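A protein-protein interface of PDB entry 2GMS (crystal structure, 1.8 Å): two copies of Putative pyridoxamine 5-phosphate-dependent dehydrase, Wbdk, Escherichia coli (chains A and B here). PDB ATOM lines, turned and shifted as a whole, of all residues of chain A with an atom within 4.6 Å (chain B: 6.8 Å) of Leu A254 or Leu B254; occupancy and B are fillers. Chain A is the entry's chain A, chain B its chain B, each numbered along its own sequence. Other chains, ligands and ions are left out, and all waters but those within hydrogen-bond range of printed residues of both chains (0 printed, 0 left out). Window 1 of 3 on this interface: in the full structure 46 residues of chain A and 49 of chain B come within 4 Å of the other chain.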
ATOM      1  N   PHE A  30     -27.869 -20.168   7.932  1.00  0.00           N
ATOM      2  CA  PHE A  30     -27.177 -19.334   8.877  1.00  0.00           C
ATOM      3  C   PHE A  30     -25.910 -19.835   9.555  1.00  0.00           C
ATOM      4  O   PHE A  30     -25.111 -19.035  10.069  1.00  0.00           O
ATOM      5  CB  PHE A  30     -28.179 -18.712   9.852  1.00  0.00           C
ATOM      6  CG  PHE A  30     -29.374 -18.136   9.122  1.00  0.00           C
ATOM      7  CD1 PHE A  30     -30.618 -18.762   9.224  1.00  0.00           C
ATOM      8  CD2 PHE A  30     -29.269 -16.985   8.334  1.00  0.00           C
ATOM      9  CE1 PHE A  30     -31.739 -18.255   8.563  1.00  0.00           C
ATOM     10  CE2 PHE A  30     -30.377 -16.454   7.671  1.00  0.00           C
ATOM     11  CZ  PHE A  30     -31.614 -17.093   7.796  1.00  0.00           C
ATOM     12  N   VAL A  36     -18.314 -18.822   4.685  1.00  0.00           N
ATOM     13  CA  VAL A  36     -17.146 -18.909   5.538  1.00  0.00           C
ATOM     14  C   VAL A  36     -15.999 -19.556   4.756  1.00  0.00           C
ATOM     15  O   VAL A  36     -14.851 -19.074   4.803  1.00  0.00           O
ATOM     16  CB  VAL A  36     -17.436 -19.559   6.897  1.00  0.00           C
ATOM     17  CG1 VAL A  36     -16.145 -20.025   7.574  1.00  0.00           C
ATOM     18  CG2 VAL A  36     -18.200 -18.597   7.814  1.00  0.00           C
ATOM     19  N   MET A 195     -18.590  -7.791  12.547  1.00  0.00           N
ATOM     20  CA  MET A 195     -19.363  -7.738  13.790  1.00  0.00           C
ATOM     21  C   MET A 195     -18.417  -8.252  14.868  1.00  0.00           C
ATOM     22  O   MET A 195     -17.892  -7.502  15.686  1.00  0.00           O
ATOM     23  CB  MET A 195     -20.697  -8.503  13.699  1.00  0.00           C
ATOM     24  CG  MET A 195     -21.557  -7.874  12.619  1.00  0.00           C
ATOM     25  SD  MET A 195     -23.174  -8.666  12.455  1.00  0.00           S
ATOM     26  CE  MET A 195     -22.683 -10.370  12.044  1.00  0.00           C
ATOM     27  N   GLU A 196     -18.140  -9.546  14.770  1.00  0.00           N
ATOM     28  CA  GLU A 196     -17.161 -10.242  15.585  1.00  0.00           C
ATOM     29  C   GLU A 196     -16.470 -11.202  14.646  1.00  0.00           C
ATOM     30  O   GLU A 196     -17.083 -11.638  13.677  1.00  0.00           O
ATOM     31  CB  GLU A 196     -17.686 -11.038  16.811  1.00  0.00           C
ATOM     32  CG  GLU A 196     -18.256 -10.126  17.909  1.00  0.00           C
ATOM     33  CD  GLU A 196     -17.473 -10.134  19.187  1.00  0.00           C
ATOM     34  OE1 GLU A 196     -16.290 -10.467  19.276  1.00  0.00           O
ATOM     35  OE2 GLU A 196     -18.211  -9.754  20.206  1.00  0.00           O
ATOM     36  N   ARG A 252     -17.230 -21.705  16.188  1.00  0.00           N
ATOM     37  CA  ARG A 252     -17.499 -21.385  14.799  1.00  0.00           C
ATOM     38  C   ARG A 252     -18.005 -19.967  14.618  1.00  0.00           C
ATOM     39  O   ARG A 252     -18.679 -19.445  15.500  1.00  0.00           O
ATOM     40  CB  ARG A 252     -18.569 -22.300  14.256  1.00  0.00           C
ATOM     41  CG  ARG A 252     -18.159 -23.760  14.133  1.00  0.00           C
ATOM     42  CD  ARG A 252     -19.333 -24.596  13.610  1.00  0.00           C
ATOM     43  NE  ARG A 252     -20.529 -24.465  14.451  1.00  0.00           N
ATOM     44  CZ  ARG A 252     -21.421 -25.431  14.700  1.00  0.00           C
ATOM     45  NH1 ARG A 252     -21.333 -26.644  14.168  1.00  0.00           N
ATOM     46  NH2 ARG A 252     -22.448 -25.181  15.505  1.00  0.00           N
ATOM     47  N   PRO A 253     -17.713 -19.357  13.462  1.00  0.00           N
ATOM     48  CA  PRO A 253     -18.222 -18.028  13.185  1.00  0.00           C
ATOM     49  C   PRO A 253     -19.577 -18.212  12.513  1.00  0.00           C
ATOM     50  O   PRO A 253     -19.927 -19.296  12.027  1.00  0.00           O
ATOM     51  CB  PRO A 253     -17.282 -17.404  12.148  1.00  0.00           C
ATOM     52  CG  PRO A 253     -16.681 -18.603  11.424  1.00  0.00           C
ATOM     53  CD  PRO A 253     -16.812 -19.792  12.363  1.00  0.00           C
ATOM     54  N   LEU A 254     -20.352 -17.148  12.465  1.00  0.00           N
ATOM     55  CA  LEU A 254     -21.634 -17.241  11.792  1.00  0.00           C
ATOM     56  C   LEU A 254     -21.411 -17.120  10.297  1.00  0.00           C
ATOM     57  O   LEU A 254     -20.493 -16.414   9.821  1.00  0.00           O
ATOM     58  CB  LEU A 254     -22.559 -16.089  12.215  1.00  0.00           C
ATOM     59  CG  LEU A 254     -23.036 -16.199  13.663  1.00  0.00           C
ATOM     60  CD1 LEU A 254     -23.971 -15.040  13.966  1.00  0.00           C
ATOM     61  CD2 LEU A 254     -23.757 -17.526  13.852  1.00  0.00           C
ATOM     62  N   GLU A 255     -22.270 -17.788   9.558  1.00  0.00           N
ATOM     63  CA  GLU A 255     -22.183 -17.689   8.117  1.00  0.00           C
ATOM     64  C   GLU A 255     -22.204 -16.221   7.649  1.00  0.00           C
ATOM     65  O   GLU A 255     -21.508 -15.834   6.705  1.00  0.00           O
ATOM     66  CB  GLU A 255     -23.318 -18.491   7.495  1.00  0.00           C
ATOM     67  CG  GLU A 255     -23.232 -18.448   5.971  1.00  0.00           C
ATOM     68  CD  GLU A 255     -22.186 -19.357   5.404  1.00  0.00           C
ATOM     69  OE1 GLU A 255     -21.150 -19.671   5.969  1.00  0.00           O
ATOM     70  OE2 GLU A 255     -22.506 -19.748   4.194  1.00  0.00           O
ATOM     71  N   MET A 256     -22.995 -15.372   8.321  1.00  0.00           N
ATOM     72  CA  MET A 256     -23.082 -13.941   7.983  1.00  0.00           C
ATOM     73  C   MET A 256     -21.737 -13.221   8.028  1.00  0.00           C
ATOM     74  O   MET A 256     -21.447 -12.363   7.184  1.00  0.00           O
ATOM     75  CB  MET A 256     -23.971 -13.162   8.964  1.00  0.00           C
ATOM     76  CG  MET A 256     -25.370 -12.972   8.463  1.00  0.00           C
ATOM     77  SD  MET A 256     -26.386 -12.306   9.778  1.00  0.00           S
ATOM     78  CE  MET A 256     -28.015 -12.853   9.199  1.00  0.00           C
ATOM     79  N   SER A 257     -20.937 -13.550   9.047  1.00  0.00           N
ATOM     80  CA  SER A 257     -19.629 -12.930   9.213  1.00  0.00           C
ATOM     81  C   SER A 257     -18.729 -13.195   8.022  1.00  0.00           C
ATOM     82  O   SER A 257     -18.049 -12.299   7.550  1.00  0.00           O
ATOM     83  CB  SER A 257     -19.028 -13.356  10.538  1.00  0.00           C
ATOM     84  OG  SER A 257     -19.845 -12.826  11.576  1.00  0.00           O
ATOM     85  N   GLY A 258     -18.754 -14.429   7.518  1.00  0.00           N
ATOM     86  CA  GLY A 258     -17.970 -14.799   6.357  1.00  0.00           C
ATOM     87  C   GLY A 258     -18.443 -14.037   5.122  1.00  0.00           C
ATOM     88  O   GLY A 258     -17.649 -13.682   4.246  1.00  0.00           O
ATOM     89  N   PHE B  30     -23.906  -3.750  16.290  1.00  0.00           N
ATOM     90  CA  PHE B  30     -23.868  -5.200  16.162  1.00  0.00           C
ATOM     91  C   PHE B  30     -23.211  -5.959  17.314  1.00  0.00           C
ATOM     92  O   PHE B  30     -23.306  -7.186  17.486  1.00  0.00           O
ATOM     93  CB  PHE B  30     -23.277  -5.568  14.779  1.00  0.00           C
ATOM     94  CG  PHE B  30     -23.883  -4.766  13.644  1.00  0.00           C
ATOM     95  CD1 PHE B  30     -23.200  -3.665  13.128  1.00  0.00           C
ATOM     96  CD2 PHE B  30     -25.122  -5.080  13.078  1.00  0.00           C
ATOM     97  CE1 PHE B  30     -23.719  -2.900  12.081  1.00  0.00           C
ATOM     98  CE2 PHE B  30     -25.659  -4.331  12.026  1.00  0.00           C
ATOM     99  CZ  PHE B  30     -24.964  -3.222  11.540  1.00  0.00           C
ATOM    100  N   THR B  31     -22.540  -5.206  18.132  1.00  0.00           N
ATOM    101  CA  THR B  31     -21.867  -5.796  19.250  1.00  0.00           C
ATOM    102  C   THR B  31     -22.834  -6.015  20.421  1.00  0.00           C
ATOM    103  O   THR B  31     -23.752  -5.217  20.665  1.00  0.00           O
ATOM    104  CB  THR B  31     -20.672  -4.849  19.563  1.00  0.00           C
ATOM    105  OG1 THR B  31     -19.715  -4.956  18.522  1.00  0.00           O
ATOM    106  CG2 THR B  31     -20.035  -5.126  20.918  1.00  0.00           C
ATOM    107  N   MET B  32     -22.610  -7.115  21.149  1.00  0.00           N
ATOM    108  CA  MET B  32     -23.390  -7.462  22.321  1.00  0.00           C
ATOM    109  C   MET B  32     -23.850  -6.213  23.084  1.00  0.00           C
ATOM    110  O   MET B  32     -23.029  -5.456  23.587  1.00  0.00           O
ATOM    111  CB  MET B  32     -22.562  -8.373  23.235  1.00  0.00           C
ATOM    112  CG  MET B  32     -23.364  -8.798  24.443  1.00  0.00           C
ATOM    113  SD  MET B  32     -22.296  -9.665  25.597  1.00  0.00           S
ATOM    114  CE  MET B  32     -21.511  -8.292  26.477  1.00  0.00           C
ATOM    115  N   GLY B  33     -25.164  -5.976  23.165  1.00  0.00           N
ATOM    116  CA  GLY B  33     -25.661  -4.793  23.853  1.00  0.00           C
ATOM    117  C   GLY B  33     -27.070  -4.925  24.443  1.00  0.00           C
ATOM    118  O   GLY B  33     -27.362  -5.845  25.217  1.00  0.00           O
ATOM    119  N   TYR B  35     -30.253  -5.608  23.168  1.00  0.00           N
ATOM    120  CA  TYR B  35     -31.073  -6.777  22.931  1.00  0.00           C
ATOM    121  C   TYR B  35     -30.620  -7.991  23.713  1.00  0.00           C
ATOM    122  O   TYR B  35     -31.435  -8.758  24.203  1.00  0.00           O
ATOM    123  CB  TYR B  35     -31.040  -7.107  21.456  1.00  0.00           C
ATOM    124  CG  TYR B  35     -31.876  -6.122  20.701  1.00  0.00           C
ATOM    125  CD1 TYR B  35     -33.256  -6.085  20.886  1.00  0.00           C
ATOM    126  CD2 TYR B  35     -31.282  -5.233  19.804  1.00  0.00           C
ATOM    127  CE1 TYR B  35     -34.038  -5.197  20.152  1.00  0.00           C
ATOM    128  CE2 TYR B  35     -32.049  -4.310  19.088  1.00  0.00           C
ATOM    129  CZ  TYR B  35     -33.440  -4.313  19.259  1.00  0.00           C
ATOM    130  OH  TYR B  35     -34.209  -3.389  18.587  1.00  0.00           O
ATOM    131  N   VAL B  36     -29.299  -8.155  23.808  1.00  0.00           N
ATOM    132  CA  VAL B  36     -28.744  -9.270  24.541  1.00  0.00           C
ATOM    133  C   VAL B  36     -29.194  -9.116  25.976  1.00  0.00           C
ATOM    134  O   VAL B  36     -29.727 -10.032  26.603  1.00  0.00           O
ATOM    135  CB  VAL B  36     -27.219  -9.393  24.383  1.00  0.00           C
ATOM    136  CG1 VAL B  36     -26.608 -10.221  25.526  1.00  0.00           C
ATOM    137  CG2 VAL B  36     -26.914 -10.035  23.021  1.00  0.00           C
ATOM    138  N   MET B  54     -26.123 -14.771  28.399  1.00  0.00           N
ATOM    139  CA  MET B  54     -26.095 -15.328  27.048  1.00  0.00           C
ATOM    140  C   MET B  54     -24.646 -15.458  26.505  1.00  0.00           C
ATOM    141  O   MET B  54     -23.820 -14.553  26.675  1.00  0.00           O
ATOM    142  CB  MET B  54     -26.940 -14.459  26.096  1.00  0.00           C
ATOM    143  CG  MET B  54     -27.079 -15.070  24.710  1.00  0.00           C
ATOM    144  SD  MET B  54     -27.799 -13.950  23.483  1.00  0.00           S
ATOM    145  CE  MET B  54     -28.212 -15.142  22.174  1.00  0.00           C
ATOM    146  N   VAL B  55     -24.312 -16.587  25.857  1.00  0.00           N
ATOM    147  CA  VAL B  55     -22.980 -16.832  25.287  1.00  0.00           C
ATOM    148  C   VAL B  55     -23.087 -17.252  23.814  1.00  0.00           C
ATOM    149  O   VAL B  55     -24.178 -17.401  23.279  1.00  0.00           O
ATOM    150  CB  VAL B  55     -22.083 -17.765  26.122  1.00  0.00           C
ATOM    151  CG1 VAL B  55     -21.748 -17.115  27.469  1.00  0.00           C
ATOM    152  CG2 VAL B  55     -22.760 -19.130  26.337  1.00  0.00           C
ATOM    153  N   SER B  56     -21.953 -17.437  23.160  1.00  0.00           N
ATOM    154  CA  SER B  56     -21.902 -17.768  21.750  1.00  0.00           C
ATOM    155  C   SER B  56     -22.509 -19.114  21.327  1.00  0.00           C
ATOM    156  O   SER B  56     -22.896 -19.312  20.165  1.00  0.00           O
ATOM    157  CB  SER B  56     -20.473 -17.575  21.225  1.00  0.00           C
ATOM    158  OG  SER B  56     -19.581 -18.496  21.849  1.00  0.00           O
ATOM    159  N   THR B 194     -31.180 -19.124  17.478  1.00  0.00           N
ATOM    160  CA  THR B 194     -30.660 -17.782  17.282  1.00  0.00           C
ATOM    161  C   THR B 194     -29.445 -17.820  16.342  1.00  0.00           C
ATOM    162  O   THR B 194     -28.580 -16.944  16.396  1.00  0.00           O
ATOM    163  CB  THR B 194     -30.322 -17.145  18.649  1.00  0.00           C
ATOM    164  OG1 THR B 194     -29.293 -17.914  19.253  1.00  0.00           O
ATOM    165  CG2 THR B 194     -31.552 -17.079  19.576  1.00  0.00           C
ATOM    166  N   MET B 195     -29.411 -18.830  15.450  1.00  0.00           N
ATOM    167  CA  MET B 195     -28.312 -19.077  14.510  1.00  0.00           C
ATOM    168  C   MET B 195     -27.345 -19.956  15.310  1.00  0.00           C
ATOM    169  O   MET B 195     -27.289 -21.177  15.138  1.00  0.00           O
ATOM    170  CB  MET B 195     -27.671 -17.792  13.889  1.00  0.00           C
ATOM    171  CG  MET B 195     -28.680 -16.944  13.121  1.00  0.00           C
ATOM    172  SD  MET B 195     -28.009 -15.509  12.225  1.00  0.00           S
ATOM    173  CE  MET B 195     -27.573 -14.370  13.560  1.00  0.00           C
ATOM    174  N   GLU B 196     -26.638 -19.324  16.249  1.00  0.00           N
ATOM    175  CA  GLU B 196     -25.778 -19.983  17.216  1.00  0.00           C
ATOM    176  C   GLU B 196     -26.121 -19.310  18.544  1.00  0.00           C
ATOM    177  O   GLU B 196     -26.559 -18.172  18.581  1.00  0.00           O
ATOM    178  CB  GLU B 196     -24.250 -19.821  16.998  1.00  0.00           C
ATOM    179  CG  GLU B 196     -23.696 -20.577  15.776  1.00  0.00           C
ATOM    180  CD  GLU B 196     -23.003 -21.857  16.142  1.00  0.00           C
ATOM    181  OE1 GLU B 196     -23.053 -22.355  17.251  1.00  0.00           O
ATOM    182  OE2 GLU B 196     -22.371 -22.397  15.131  1.00  0.00           O
ATOM    183  N   GLY B 197     -25.908 -19.971  19.644  1.00  0.00           N
ATOM    184  CA  GLY B 197     -26.211 -19.279  20.865  1.00  0.00           C
ATOM    185  C   GLY B 197     -26.363 -20.251  22.021  1.00  0.00           C
ATOM    186  O   GLY B 197     -26.697 -21.431  21.850  1.00  0.00           O
ATOM    187  N   ARG B 252     -18.633 -13.733  23.643  1.00  0.00           N
ATOM    188  CA  ARG B 252     -19.812 -12.919  23.557  1.00  0.00           C
ATOM    189  C   ARG B 252     -20.686 -13.371  22.397  1.00  0.00           C
ATOM    190  O   ARG B 252     -20.159 -13.808  21.369  1.00  0.00           O
ATOM    191  CB  ARG B 252     -19.373 -11.511  23.252  1.00  0.00           C
ATOM    192  CG  ARG B 252     -18.812 -10.805  24.450  1.00  0.00           C
ATOM    193  CD  ARG B 252     -18.678  -9.352  24.046  1.00  0.00           C
ATOM    194  NE  ARG B 252     -17.795  -9.300  22.903  1.00  0.00           N
ATOM    195  CZ  ARG B 252     -16.836  -8.404  22.772  1.00  0.00           C
ATOM    196  NH1 ARG B 252     -16.653  -7.457  23.691  1.00  0.00           N
ATOM    197  NH2 ARG B 252     -16.040  -8.455  21.698  1.00  0.00           N
ATOM    198  N   PRO B 253     -22.016 -13.244  22.569  1.00  0.00           N
ATOM    199  CA  PRO B 253     -22.949 -13.571  21.501  1.00  0.00           C
ATOM    200  C   PRO B 253     -23.129 -12.297  20.645  1.00  0.00           C
ATOM    201  O   PRO B 253     -22.693 -11.214  21.032  1.00  0.00           O
ATOM    202  CB  PRO B 253     -24.288 -13.902  22.187  1.00  0.00           C
ATOM    203  CG  PRO B 253     -24.246 -13.153  23.514  1.00  0.00           C
ATOM    204  CD  PRO B 253     -22.758 -13.019  23.846  1.00  0.00           C
ATOM    205  N   LEU B 254     -23.760 -12.402  19.485  1.00  0.00           N
ATOM    206  CA  LEU B 254     -23.991 -11.211  18.683  1.00  0.00           C
ATOM    207  C   LEU B 254     -25.320 -10.568  19.062  1.00  0.00           C
ATOM    208  O   LEU B 254     -26.267 -11.215  19.536  1.00  0.00           O
ATOM    209  CB  LEU B 254     -23.938 -11.489  17.174  1.00  0.00           C
ATOM    210  CG  LEU B 254     -22.542 -11.805  16.654  1.00  0.00           C
ATOM    211  CD1 LEU B 254     -22.657 -12.252  15.202  1.00  0.00           C
ATOM    212  CD2 LEU B 254     -21.669 -10.558  16.771  1.00  0.00           C
ATOM    213  N   GLU B 255     -25.396  -9.264  18.860  1.00  0.00           N
ATOM    214  CA  GLU B 255     -26.626  -8.573  19.184  1.00  0.00           C
ATOM    215  C   GLU B 255     -27.791  -9.193  18.418  1.00  0.00           C
ATOM    216  O   GLU B 255     -28.889  -9.342  18.948  1.00  0.00           O
ATOM    217  CB  GLU B 255     -26.473  -7.077  18.861  1.00  0.00           C
ATOM    218  CG  GLU B 255     -27.614  -6.206  19.394  1.00  0.00           C
ATOM    219  CD  GLU B 255     -27.629  -5.968  20.882  1.00  0.00           C
ATOM    220  OE1 GLU B 255     -27.056  -6.664  21.703  1.00  0.00           O
ATOM    221  OE2 GLU B 255     -28.361  -4.941  21.224  1.00  0.00           O
ATOM    222  N   MET B 256     -27.538  -9.555  17.160  1.00  0.00           N
ATOM    223  CA  MET B 256     -28.574 -10.174  16.347  1.00  0.00           C
ATOM    224  C   MET B 256     -29.175 -11.392  17.011  1.00  0.00           C
ATOM    225  O   MET B 256     -30.373 -11.613  16.982  1.00  0.00           O
ATOM    226  CB  MET B 256     -28.030 -10.712  15.019  1.00  0.00           C
ATOM    227  CG  MET B 256     -28.370  -9.839  13.828  1.00  0.00           C
ATOM    228  SD  MET B 256     -27.320 -10.215  12.409  1.00  0.00           S
ATOM    229  CE  MET B 256     -27.152  -8.574  11.682  1.00  0.00           C
ATOM    230  N   SER B 257     -28.325 -12.224  17.574  1.00  0.00           N
ATOM    231  CA  SER B 257     -28.812 -13.424  18.209  1.00  0.00           C
ATOM    232  C   SER B 257     -29.719 -13.078  19.366  1.00  0.00           C
ATOM    233  O   SER B 257     -30.727 -13.754  19.596  1.00  0.00           O
ATOM    234  CB  SER B 257     -27.661 -14.302  18.671  1.00  0.00           C
ATOM    235  OG  SER B 257     -26.863 -14.619  17.542  1.00  0.00           O
ATOM    236  N   GLY B 258     -29.326 -12.029  20.089  1.00  0.00           N
ATOM    237  CA  GLY B 258     -30.123 -11.593  21.213  1.00  0.00           C
ATOM    238  C   GLY B 258     -31.509 -11.133  20.744  1.00  0.00           C
ATOM    239  O   GLY B 258     -32.509 -11.524  21.316  1.00  0.00           O
ATOM    240  N   ALA B 259     -31.567 -10.305  19.694  1.00  0.00           N
ATOM    241  CA  ALA B 259     -32.822  -9.772  19.167  1.00  0.00           C
ATOM    242  C   ALA B 259     -33.757 -10.880  18.664  1.00  0.00           C
ATOM    243  O   ALA B 259     -34.975 -10.820  18.865  1.00  0.00           O
ATOM    244  CB  ALA B 259     -32.542  -8.756  18.066  1.00  0.00           C
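The backbone carbonyl oxygen of Phe A30 is in hydrogen-bond range of the backbone NH of Glu A255, at 3.1 Å. The backbone NH (N) of Glu B255 is in hydrogen-bond range of the backbone carbonyl oxygen (O) of Phe B30. The backbone carbonyl oxygen (O) of Glu B196 is in hydrogen-bond range of the side-chain hydroxyl (OG1) of Thr B194 (2.8 Å).
Printed residues of chain A within 4 Å of Met B195: Phe A30 (3.8 Å) and Leu A254 (3.7 Å). Printed residues of chain B within 4 Å of Glu A196: Arg B252 (2.8 Å) and Leu B254 (3.6 Å). Printed residues of chain A within 4 Å of Arg B252: Glu A196 (2.8 Å). Glu B255 touches none of the printed residues of chain A. Ala B259 touches none of the printed residues of chain A. The nearest residue of chain B that does not touch Leu A254 is Ser B257 (4.6 Å).
NE of Arg B252 is in salt-bridge range of OE2 of Glu A196 (2.8 Å). The guanidinium group (NH2) of Arg A252 is in salt-bridge range of the side-chain carboxylate (OE2) of Glu B196, 2.8 Å away. SD of Met A256 lies close to SD of Met B256 (3.5 Å).
Met A195 touches Leu B254, and with the chains exchanged Leu A254 touches Met B195. Glu A196 touches Leu B254, and with the chains exchanged Leu A254 touches Glu B196. Leu B254 touches its own counterpart, Leu A254. Met A256 touches its own counterpart, Met B256.
Among the printed residues, pairs that only touch across the chains: Phe A30 with Met B195, Met A195 with Phe B30, Met A195 with Leu B254, Glu A196 with Leu B254, Leu A254 with Met B195, Leu A254 with Glu B196 and Leu A254 with Leu B254.
Of the 21 printed residues of chain B, 6 touch a printed residue of chain A. Hydrophobic or aromatic side chains of chain B that line the printed part of chain A: Phe B30, Met B195, Leu B254 and Met B256. Among the printed residues, 10 pairs touch across the chains. Among the printed residues, Asp or Glu carboxylates within 4 Å of a Lys or Arg side-chain nitrogen of the other chain: Glu A196 with Arg B252 and Arg A252 with Glu B196.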
